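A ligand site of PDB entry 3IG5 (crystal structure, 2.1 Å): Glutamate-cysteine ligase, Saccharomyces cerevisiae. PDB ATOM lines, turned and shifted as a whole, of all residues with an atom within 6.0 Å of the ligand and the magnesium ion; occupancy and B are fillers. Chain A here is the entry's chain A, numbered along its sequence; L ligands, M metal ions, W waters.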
ATOM      1  N   GLU A  50     -16.603  -7.013  23.949  1.00  0.00           N
ATOM      2  CA  GLU A  50     -15.654  -6.270  23.172  1.00  0.00           C
ATOM      3  C   GLU A  50     -16.530  -5.347  22.302  1.00  0.00           C
ATOM      4  O   GLU A  50     -17.353  -5.850  21.492  1.00  0.00           O
ATOM      5  CB  GLU A  50     -14.911  -7.287  22.362  1.00  0.00           C
ATOM      6  CG  GLU A  50     -13.618  -6.840  21.748  1.00  0.00           C
ATOM      7  CD  GLU A  50     -12.784  -8.065  21.269  1.00  0.00           C
ATOM      8  OE1 GLU A  50     -12.161  -7.957  20.191  1.00  0.00           O
ATOM      9  OE2 GLU A  50     -12.767  -9.116  21.971  1.00  0.00           O
ATOM     10  N   GLU A  52     -16.857  -1.855  19.608  1.00  0.00           N
ATOM     11  CA  GLU A  52     -16.133  -0.992  18.738  1.00  0.00           C
ATOM     12  C   GLU A  52     -16.897   0.302  18.534  1.00  0.00           C
ATOM     13  O   GLU A  52     -18.137   0.295  18.403  1.00  0.00           O
ATOM     14  CB  GLU A  52     -15.859  -1.741  17.423  1.00  0.00           C
ATOM     15  CG  GLU A  52     -14.933  -2.906  17.655  1.00  0.00           C
ATOM     16  CD  GLU A  52     -14.954  -3.934  16.572  1.00  0.00           C
ATOM     17  OE1 GLU A  52     -15.908  -3.923  15.764  1.00  0.00           O
ATOM     18  OE2 GLU A  52     -13.999  -4.754  16.529  1.00  0.00           O
ATOM     19  N   GLU A  96      -8.258  -0.864  16.076  1.00  0.00           N
ATOM     20  CA  GLU A  96      -8.994  -1.649  15.105  1.00  0.00           C
ATOM     21  C   GLU A  96      -8.633  -1.196  13.685  1.00  0.00           C
ATOM     22  O   GLU A  96      -7.904  -0.211  13.512  1.00  0.00           O
ATOM     23  CB  GLU A  96     -10.499  -1.600  15.338  1.00  0.00           C
ATOM     24  CG  GLU A  96     -11.108  -2.937  15.785  1.00  0.00           C
ATOM     25  CD  GLU A  96     -10.758  -4.176  14.898  1.00  0.00           C
ATOM     26  OE1 GLU A  96     -10.577  -4.088  13.634  1.00  0.00           O
ATOM     27  OE2 GLU A  96     -10.659  -5.281  15.479  1.00  0.00           O
ATOM     28  N   MET A 101     -11.680   4.325  14.367  1.00  0.00           N
ATOM     29  CA  MET A 101     -12.304   3.392  15.281  1.00  0.00           C
ATOM     30  C   MET A 101     -11.522   3.300  16.575  1.00  0.00           C
ATOM     31  O   MET A 101     -10.281   3.520  16.607  1.00  0.00           O
ATOM     32  CB  MET A 101     -12.379   1.990  14.686  1.00  0.00           C
ATOM     33  CG  MET A 101     -13.250   1.887  13.450  1.00  0.00           C
ATOM     34  SD  MET A 101     -13.177   0.320  12.620  1.00  0.00           S
ATOM     35  CE  MET A 101     -14.261  -0.723  13.570  1.00  0.00           C
ATOM     36  N   GLU A 103     -11.545   0.377  19.906  1.00  0.00           N
ATOM     37  CA  GLU A 103     -12.138  -0.831  20.462  1.00  0.00           C
ATOM     38  C   GLU A 103     -11.846  -0.807  21.946  1.00  0.00           C
ATOM     39  O   GLU A 103     -10.770  -0.329  22.342  1.00  0.00           O
ATOM     40  CB  GLU A 103     -11.528  -2.065  19.814  1.00  0.00           C
ATOM     41  CG  GLU A 103     -11.889  -3.384  20.489  1.00  0.00           C
ATOM     42  CD  GLU A 103     -11.297  -4.560  19.703  1.00  0.00           C
ATOM     43  OE1 GLU A 103     -11.716  -4.744  18.519  1.00  0.00           O
ATOM     44  OE2 GLU A 103     -10.386  -5.260  20.224  1.00  0.00           O
ATOM     45  N   GLY A 261     -15.805  -3.025   5.099  1.00  0.00           N
ATOM     46  CA  GLY A 261     -16.223  -4.135   5.921  1.00  0.00           C
ATOM     47  C   GLY A 261     -15.489  -4.095   7.246  1.00  0.00           C
ATOM     48  O   GLY A 261     -16.091  -3.992   8.290  1.00  0.00           O
ATOM     49  N   MET A 262     -14.167  -4.156   7.224  1.00  0.00           N
ATOM     50  CA  MET A 262     -13.453  -4.089   8.487  1.00  0.00           C
ATOM     51  C   MET A 262     -13.496  -2.713   9.079  1.00  0.00           C
ATOM     52  O   MET A 262     -13.080  -2.534  10.214  1.00  0.00           O
ATOM     53  CB  MET A 262     -12.037  -4.581   8.332  1.00  0.00           C
ATOM     54  CG  MET A 262     -11.991  -6.073   8.048  1.00  0.00           C
ATOM     55  SD  MET A 262     -12.287  -6.947   9.619  1.00  0.00           S
ATOM     56  CE  MET A 262     -11.820  -8.668   9.226  1.00  0.00           C
ATOM     57  N   CYS A 264     -16.414  -1.476   9.650  1.00  0.00           N
ATOM     58  CA  CYS A 264     -17.719  -1.590  10.321  1.00  0.00           C
ATOM     59  C   CYS A 264     -17.490  -2.121  11.718  1.00  0.00           C
ATOM     60  O   CYS A 264     -16.431  -2.707  11.977  1.00  0.00           O
ATOM     61  CB  CYS A 264     -18.571  -2.600   9.598  1.00  0.00           C
ATOM     62  SG  CYS A 264     -19.414  -1.840   8.189  1.00  0.00           S
ATOM     63  N   SER A 265     -18.449  -1.937  12.628  1.00  0.00           N
ATOM     64  CA  SER A 265     -18.257  -2.334  14.029  1.00  0.00           C
ATOM     65  C   SER A 265     -19.230  -3.433  14.521  1.00  0.00           C
ATOM     66  O   SER A 265     -20.330  -3.576  13.972  1.00  0.00           O
ATOM     67  CB  SER A 265     -18.397  -1.117  14.929  1.00  0.00           C
ATOM     68  OG  SER A 265     -17.373  -0.195  14.641  1.00  0.00           O
ATOM     69  N   CYS A 266     -18.848  -4.157  15.581  1.00  0.00           N
ATOM     70  CA  CYS A 266     -19.678  -5.240  16.086  1.00  0.00           C
ATOM     71  C   CYS A 266     -19.580  -5.320  17.575  1.00  0.00           C
ATOM     72  O   CYS A 266     -18.706  -4.697  18.196  1.00  0.00           O
ATOM     73  CB  CYS A 266     -19.297  -6.603  15.473  1.00  0.00           C
ATOM     74  SG  CYS A 266     -17.599  -7.154  15.894  1.00  0.00           S
ATOM     75  N   GLN A 268     -18.842  -8.268  20.309  1.00  0.00           N
ATOM     76  CA  GLN A 268     -18.385  -9.641  20.381  1.00  0.00           C
ATOM     77  C   GLN A 268     -18.298 -10.057  21.865  1.00  0.00           C
ATOM     78  O   GLN A 268     -17.966  -9.209  22.703  1.00  0.00           O
ATOM     79  CB  GLN A 268     -17.014  -9.801  19.735  1.00  0.00           C
ATOM     80  CG  GLN A 268     -17.056  -9.648  18.253  1.00  0.00           C
ATOM     81  CD  GLN A 268     -15.674  -9.669  17.603  1.00  0.00           C
ATOM     82  OE1 GLN A 268     -14.644  -9.684  18.275  1.00  0.00           O
ATOM     83  NE2 GLN A 268     -15.641  -9.720  16.279  1.00  0.00           N
ATOM     84  N   ARG A 313     -24.420  -6.280   8.297  1.00  0.00           N
ATOM     85  CA  ARG A 313     -23.143  -5.984   7.692  1.00  0.00           C
ATOM     86  C   ARG A 313     -22.428  -7.239   7.187  1.00  0.00           C
ATOM     87  O   ARG A 313     -21.358  -7.128   6.483  1.00  0.00           O
ATOM     88  CB  ARG A 313     -22.237  -5.406   8.811  1.00  0.00           C
ATOM     89  CG  ARG A 313     -21.618  -6.543   9.682  1.00  0.00           C
ATOM     90  CD  ARG A 313     -21.221  -6.048  11.089  1.00  0.00           C
ATOM     91  NE  ARG A 313     -20.579  -7.120  11.888  1.00  0.00           N
ATOM     92  CZ  ARG A 313     -21.224  -8.061  12.541  1.00  0.00           C
ATOM     93  NH1 ARG A 313     -22.561  -8.105  12.457  1.00  0.00           N
ATOM     94  NH2 ARG A 313     -20.541  -8.954  13.282  1.00  0.00           N
ATOM     95  N   TRP A 314     -22.931  -8.417   7.598  1.00  0.00           N
ATOM     96  CA  TRP A 314     -22.094  -9.637   7.582  1.00  0.00           C
ATOM     97  C   TRP A 314     -21.462  -9.878   6.202  1.00  0.00           C
ATOM     98  O   TRP A 314     -20.223 -10.060   6.080  1.00  0.00           O
ATOM     99  CB  TRP A 314     -22.857 -10.887   8.009  1.00  0.00           C
ATOM    100  CG  TRP A 314     -21.938 -12.104   8.094  1.00  0.00           C
ATOM    101  CD1 TRP A 314     -21.706 -13.048   7.134  1.00  0.00           C
ATOM    102  CD2 TRP A 314     -21.122 -12.473   9.219  1.00  0.00           C
ATOM    103  NE1 TRP A 314     -20.750 -13.974   7.571  1.00  0.00           N
ATOM    104  CE2 TRP A 314     -20.399 -13.646   8.855  1.00  0.00           C
ATOM    105  CE3 TRP A 314     -20.952 -11.926  10.507  1.00  0.00           C
ATOM    106  CZ2 TRP A 314     -19.494 -14.277   9.736  1.00  0.00           C
ATOM    107  CZ3 TRP A 314     -20.017 -12.532  11.371  1.00  0.00           C
ATOM    108  CH2 TRP A 314     -19.313 -13.700  10.967  1.00  0.00           C
ATOM    109  N   ILE A 317     -18.493  -7.449   5.282  1.00  0.00           N
ATOM    110  CA  ILE A 317     -17.222  -7.816   5.871  1.00  0.00           C
ATOM    111  C   ILE A 317     -16.650  -9.115   5.288  1.00  0.00           C
ATOM    112  O   ILE A 317     -15.399  -9.275   5.189  1.00  0.00           O
ATOM    113  CB  ILE A 317     -17.277  -7.919   7.381  1.00  0.00           C
ATOM    114  CG1 ILE A 317     -18.251  -6.882   7.934  1.00  0.00           C
ATOM    115  CG2 ILE A 317     -15.805  -7.837   7.953  1.00  0.00           C
ATOM    116  CD1 ILE A 317     -17.960  -6.429   9.352  1.00  0.00           C
ATOM    117  N   TYR A 362     -13.422 -14.912   5.868  1.00  0.00           N
ATOM    118  CA  TYR A 362     -14.334 -14.253   6.799  1.00  0.00           C
ATOM    119  C   TYR A 362     -15.707 -14.851   6.446  1.00  0.00           C
ATOM    120  O   TYR A 362     -16.298 -14.507   5.409  1.00  0.00           O
ATOM    121  CB  TYR A 362     -14.277 -12.712   6.641  1.00  0.00           C
ATOM    122  CG  TYR A 362     -15.101 -11.976   7.704  1.00  0.00           C
ATOM    123  CD1 TYR A 362     -14.512 -11.184   8.676  1.00  0.00           C
ATOM    124  CD2 TYR A 362     -16.469 -12.178   7.770  1.00  0.00           C
ATOM    125  CE1 TYR A 362     -15.326 -10.544   9.692  1.00  0.00           C
ATOM    126  CE2 TYR A 362     -17.264 -11.580   8.723  1.00  0.00           C
ATOM    127  CZ  TYR A 362     -16.698 -10.782   9.692  1.00  0.00           C
ATOM    128  OH  TYR A 362     -17.581 -10.187  10.627  1.00  0.00           O
ATOM    129  N   SER A 442      -6.222 -16.192  13.733  1.00  0.00           N
ATOM    130  CA  SER A 442      -6.758 -14.856  13.833  1.00  0.00           C
ATOM    131  C   SER A 442      -7.283 -14.276  12.519  1.00  0.00           C
ATOM    132  O   SER A 442      -8.008 -13.292  12.537  1.00  0.00           O
ATOM    133  CB  SER A 442      -5.743 -13.912  14.505  1.00  0.00           C
ATOM    134  OG  SER A 442      -4.762 -13.541  13.537  1.00  0.00           O
ATOM    135  N   TRP A 445     -12.109 -15.598  10.239  1.00  0.00           N
ATOM    136  CA  TRP A 445     -13.011 -14.733  11.005  1.00  0.00           C
ATOM    137  C   TRP A 445     -14.421 -15.302  10.878  1.00  0.00           C
ATOM    138  O   TRP A 445     -15.030 -15.170   9.839  1.00  0.00           O
ATOM    139  CB  TRP A 445     -13.051 -13.319  10.404  1.00  0.00           C
ATOM    140  CG  TRP A 445     -11.826 -12.471  10.560  1.00  0.00           C
ATOM    141  CD1 TRP A 445     -11.477 -11.712  11.613  1.00  0.00           C
ATOM    142  CD2 TRP A 445     -10.811 -12.261   9.561  1.00  0.00           C
ATOM    143  NE1 TRP A 445     -10.289 -11.075  11.381  1.00  0.00           N
ATOM    144  CE2 TRP A 445      -9.888 -11.347  10.094  1.00  0.00           C
ATOM    145  CE3 TRP A 445     -10.626 -12.752   8.240  1.00  0.00           C
ATOM    146  CZ2 TRP A 445      -8.734 -10.909   9.375  1.00  0.00           C
ATOM    147  CZ3 TRP A 445      -9.490 -12.336   7.512  1.00  0.00           C
ATOM    148  CH2 TRP A 445      -8.551 -11.403   8.100  1.00  0.00           C
ATOM    149  N   ARG A 449     -15.720 -18.416  17.425  1.00  0.00           N
ATOM    150  CA  ARG A 449     -14.324 -18.790  17.344  1.00  0.00           C
ATOM    151  C   ARG A 449     -14.014 -19.688  18.543  1.00  0.00           C
ATOM    152  O   ARG A 449     -14.378 -19.375  19.693  1.00  0.00           O
ATOM    153  CB  ARG A 449     -13.422 -17.569  17.366  1.00  0.00           C
ATOM    154  CG  ARG A 449     -11.939 -17.896  17.234  1.00  0.00           C
ATOM    155  CD  ARG A 449     -11.090 -16.625  17.108  1.00  0.00           C
ATOM    156  NE  ARG A 449     -11.237 -16.120  15.748  1.00  0.00           N
ATOM    157  CZ  ARG A 449     -10.696 -14.988  15.313  1.00  0.00           C
ATOM    158  NH1 ARG A 449      -9.996 -14.203  16.126  1.00  0.00           N
ATOM    159  NH2 ARG A 449     -10.870 -14.672  14.073  1.00  0.00           N
ATOM    160  N   ARG A 472     -19.459 -14.120  17.824  1.00  0.00           N
ATOM    161  CA  ARG A 472     -19.034 -12.972  17.023  1.00  0.00           C
ATOM    162  C   ARG A 472     -20.074 -12.281  16.089  1.00  0.00           C
ATOM    163  O   ARG A 472     -19.719 -11.283  15.427  1.00  0.00           O
ATOM    164  CB  ARG A 472     -17.817 -13.363  16.193  1.00  0.00           C
ATOM    165  CG  ARG A 472     -16.643 -13.772  17.062  1.00  0.00           C
ATOM    166  CD  ARG A 472     -15.683 -14.576  16.295  1.00  0.00           C
ATOM    167  NE  ARG A 472     -15.232 -13.806  15.135  1.00  0.00           N
ATOM    168  CZ  ARG A 472     -14.223 -12.929  15.144  1.00  0.00           C
ATOM    169  NH1 ARG A 472     -13.489 -12.754  16.240  1.00  0.00           N
ATOM    170  NH2 ARG A 472     -13.940 -12.230  14.051  1.00  0.00           N
ATOM    171  N   PHE A 474     -23.063 -10.493  16.621  1.00  0.00           N
ATOM    172  CA  PHE A 474     -23.889  -9.336  16.928  1.00  0.00           C
ATOM    173  C   PHE A 474     -23.444  -8.030  16.191  1.00  0.00           C
ATOM    174  O   PHE A 474     -22.285  -7.705  16.220  1.00  0.00           O
ATOM    175  CB  PHE A 474     -23.844  -9.025  18.411  1.00  0.00           C
ATOM    176  CG  PHE A 474     -24.763  -9.884  19.315  1.00  0.00           C
ATOM    177  CD1 PHE A 474     -26.042 -10.143  18.998  1.00  0.00           C
ATOM    178  CD2 PHE A 474     -24.269 -10.363  20.542  1.00  0.00           C
ATOM    179  CE1 PHE A 474     -26.894 -10.829  19.941  1.00  0.00           C
ATOM    180  CE2 PHE A 474     -25.055 -11.072  21.445  1.00  0.00           C
ATOM    181  CZ  PHE A 474     -26.369 -11.333  21.134  1.00  0.00           C
HETATM  182  N1  LIG L   1     -15.258  -5.359  13.146  1.00  0.00           N
HETATM  183  C1  LIG L   1     -15.518  -6.771  12.730  1.00  0.00           C
HETATM  184  C2  LIG L   1     -17.039  -7.046  12.776  1.00  0.00           C
HETATM  185  O1  LIG L   1     -17.882  -6.146  12.641  1.00  0.00           O
HETATM  186  C3  LIG L   1     -14.791  -7.756  13.643  1.00  0.00           C
HETATM  187  C4  LIG L   1     -13.286  -8.052  13.360  1.00  0.00           C
HETATM  188  C5  LIG L   1     -12.579  -8.520  14.640  1.00  0.00           C
HETATM  189  O2  LIG L   1     -12.732  -7.779  15.652  1.00  0.00           O
HETATM  190  O3  LIG L   1     -11.890  -9.609  14.686  1.00  0.00           O
HETATM  191  O4  LIG L   1     -17.469  -8.193  12.941  1.00  0.00           O
HETATM  192 MG    MG M   1     -12.498  -6.196  17.120  1.00  0.00          MG
HETATM  193  O   HOH W   1     -17.636 -10.388  14.370  1.00  0.00           O
HETATM  194  O   HOH W   2      -9.243 -11.886  14.463  1.00  0.00           O
HETATM  195  O   HOH W   3     -11.284  -9.936  17.170  1.00  0.00           O
HETATM  196  O   HOH W   4     -10.785  -7.437  18.149  1.00  0.00           O
HETATM  197  O   HOH W   5      -9.324  -8.463  12.984  1.00  0.00           O
HETATM  198  O   HOH W   6     -12.955  -4.169  12.284  1.00  0.00           O
HETATM  199  O   HOH W   7     -13.768  -6.797  18.418  1.00  0.00           O
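OE1 of Glu 50 touches the magnesium ion (3.6 Å). Of the 20 residues printed, 4 come within 4 Å of the magnesium ion. The nearest printed residue that does not touch the magnesium ion is Gln 268 (4.3 Å).
The magnesium ion is bound by water W7 (1.9 Å). OE1 of Glu 103 is bound to the magnesium ion (2.2 Å). The magnesium ion is bound by OE2 of Glu 52 (2.2 Å). O2 of the ligand binds the magnesium ion (2.2 Å). The magnesium ion is bound by water W4 (2.4 Å). Slightly farther from the magnesium ion lies the side-chain carboxylate (OE2) of Glu 96 (2.6 Å).
NH2 of Arg 313 lies within hydrogen-bond range of O of Arg 472, 3.3 Å away. O of Ser 442 lies within hydrogen-bond range of NE1 of Trp 445, at 3.4 Å. The backbone carbonyl oxygen of Gln 268 sits at hydrogen-bond distance from the backbone NH of Glu 50, at 2.9 Å. OE1 of Glu 52 is in hydrogen-bond range of N of Cys 266, 3.0 Å away. The side-chain sulfur (SG) of Cys 266 sits at hydrogen-bond distance from the side-chain amide nitrogen (NE2) of Gln 268.
Water W7 bridges OE1 of Glu 50 (2.7 Å) and OE1 of Gln 268 (3.0 Å). Water W1 lies within hydrogen-bond range of O of Arg 472 (2.5 Å), O4 of the ligand (2.6 Å), NE2 of Gln 268 (2.8 Å), NH2 of Arg 313 (3.4 Å) and SG of Cys 266 (3.6 Å). Water W6 lies within hydrogen-bond range of the backbone carbonyl oxygen of Met 262 (2.6 Å), a nitrogen (N1) of the ligand (2.7 Å) and the side-chain carboxylate of Glu 96 (2.7 Å). Water W5 lies within hydrogen-bond range of the indole nitrogen of Trp 445 and an oxygen (O3) of the ligand. Water W2 lies within hydrogen-bond range of O of Ser 442, NH1 of Arg 449, NE1 of Trp 445 and O3 of the ligand.
Ser 265 touches the ligand. NE2 of Gln 268 touches C3 of the ligand (3.4 Å). Ile 317 touches the ligand. Trp 445 touches the ligand (CD1 to O3, 3.7 Å). Hydrophobic or aromatic side chains that line the ligand: Ile 317 and Trp 445. 11 residues have an atom within 4 Å of the ligand: Glu 52, Glu 96, Cys 264, Ser 265, Cys 266, Gln 268, Arg 313, Ile 317, Tyr 362, Trp 445 and Arg 472.
An oxygen (O4) of the ligand is in hydrogen-bond range of the side-chain hydroxyl of Tyr 362. NH2 of Arg 472 is in salt-bridge range of O3 of the ligand, 3.4 Å away. The guanidinium group (NE) of Arg 313 lies within salt-bridge range of an oxygen (O1) of the ligand, at 3.0 Å. The backbone carbonyl oxygen (O) of Cys 264 lies within hydrogen-bond range of a nitrogen (N1) of the ligand (3.1 Å). SG of Cys 266 is in hydrogen-bond range of O4 of the ligand, at 3.1 Å.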
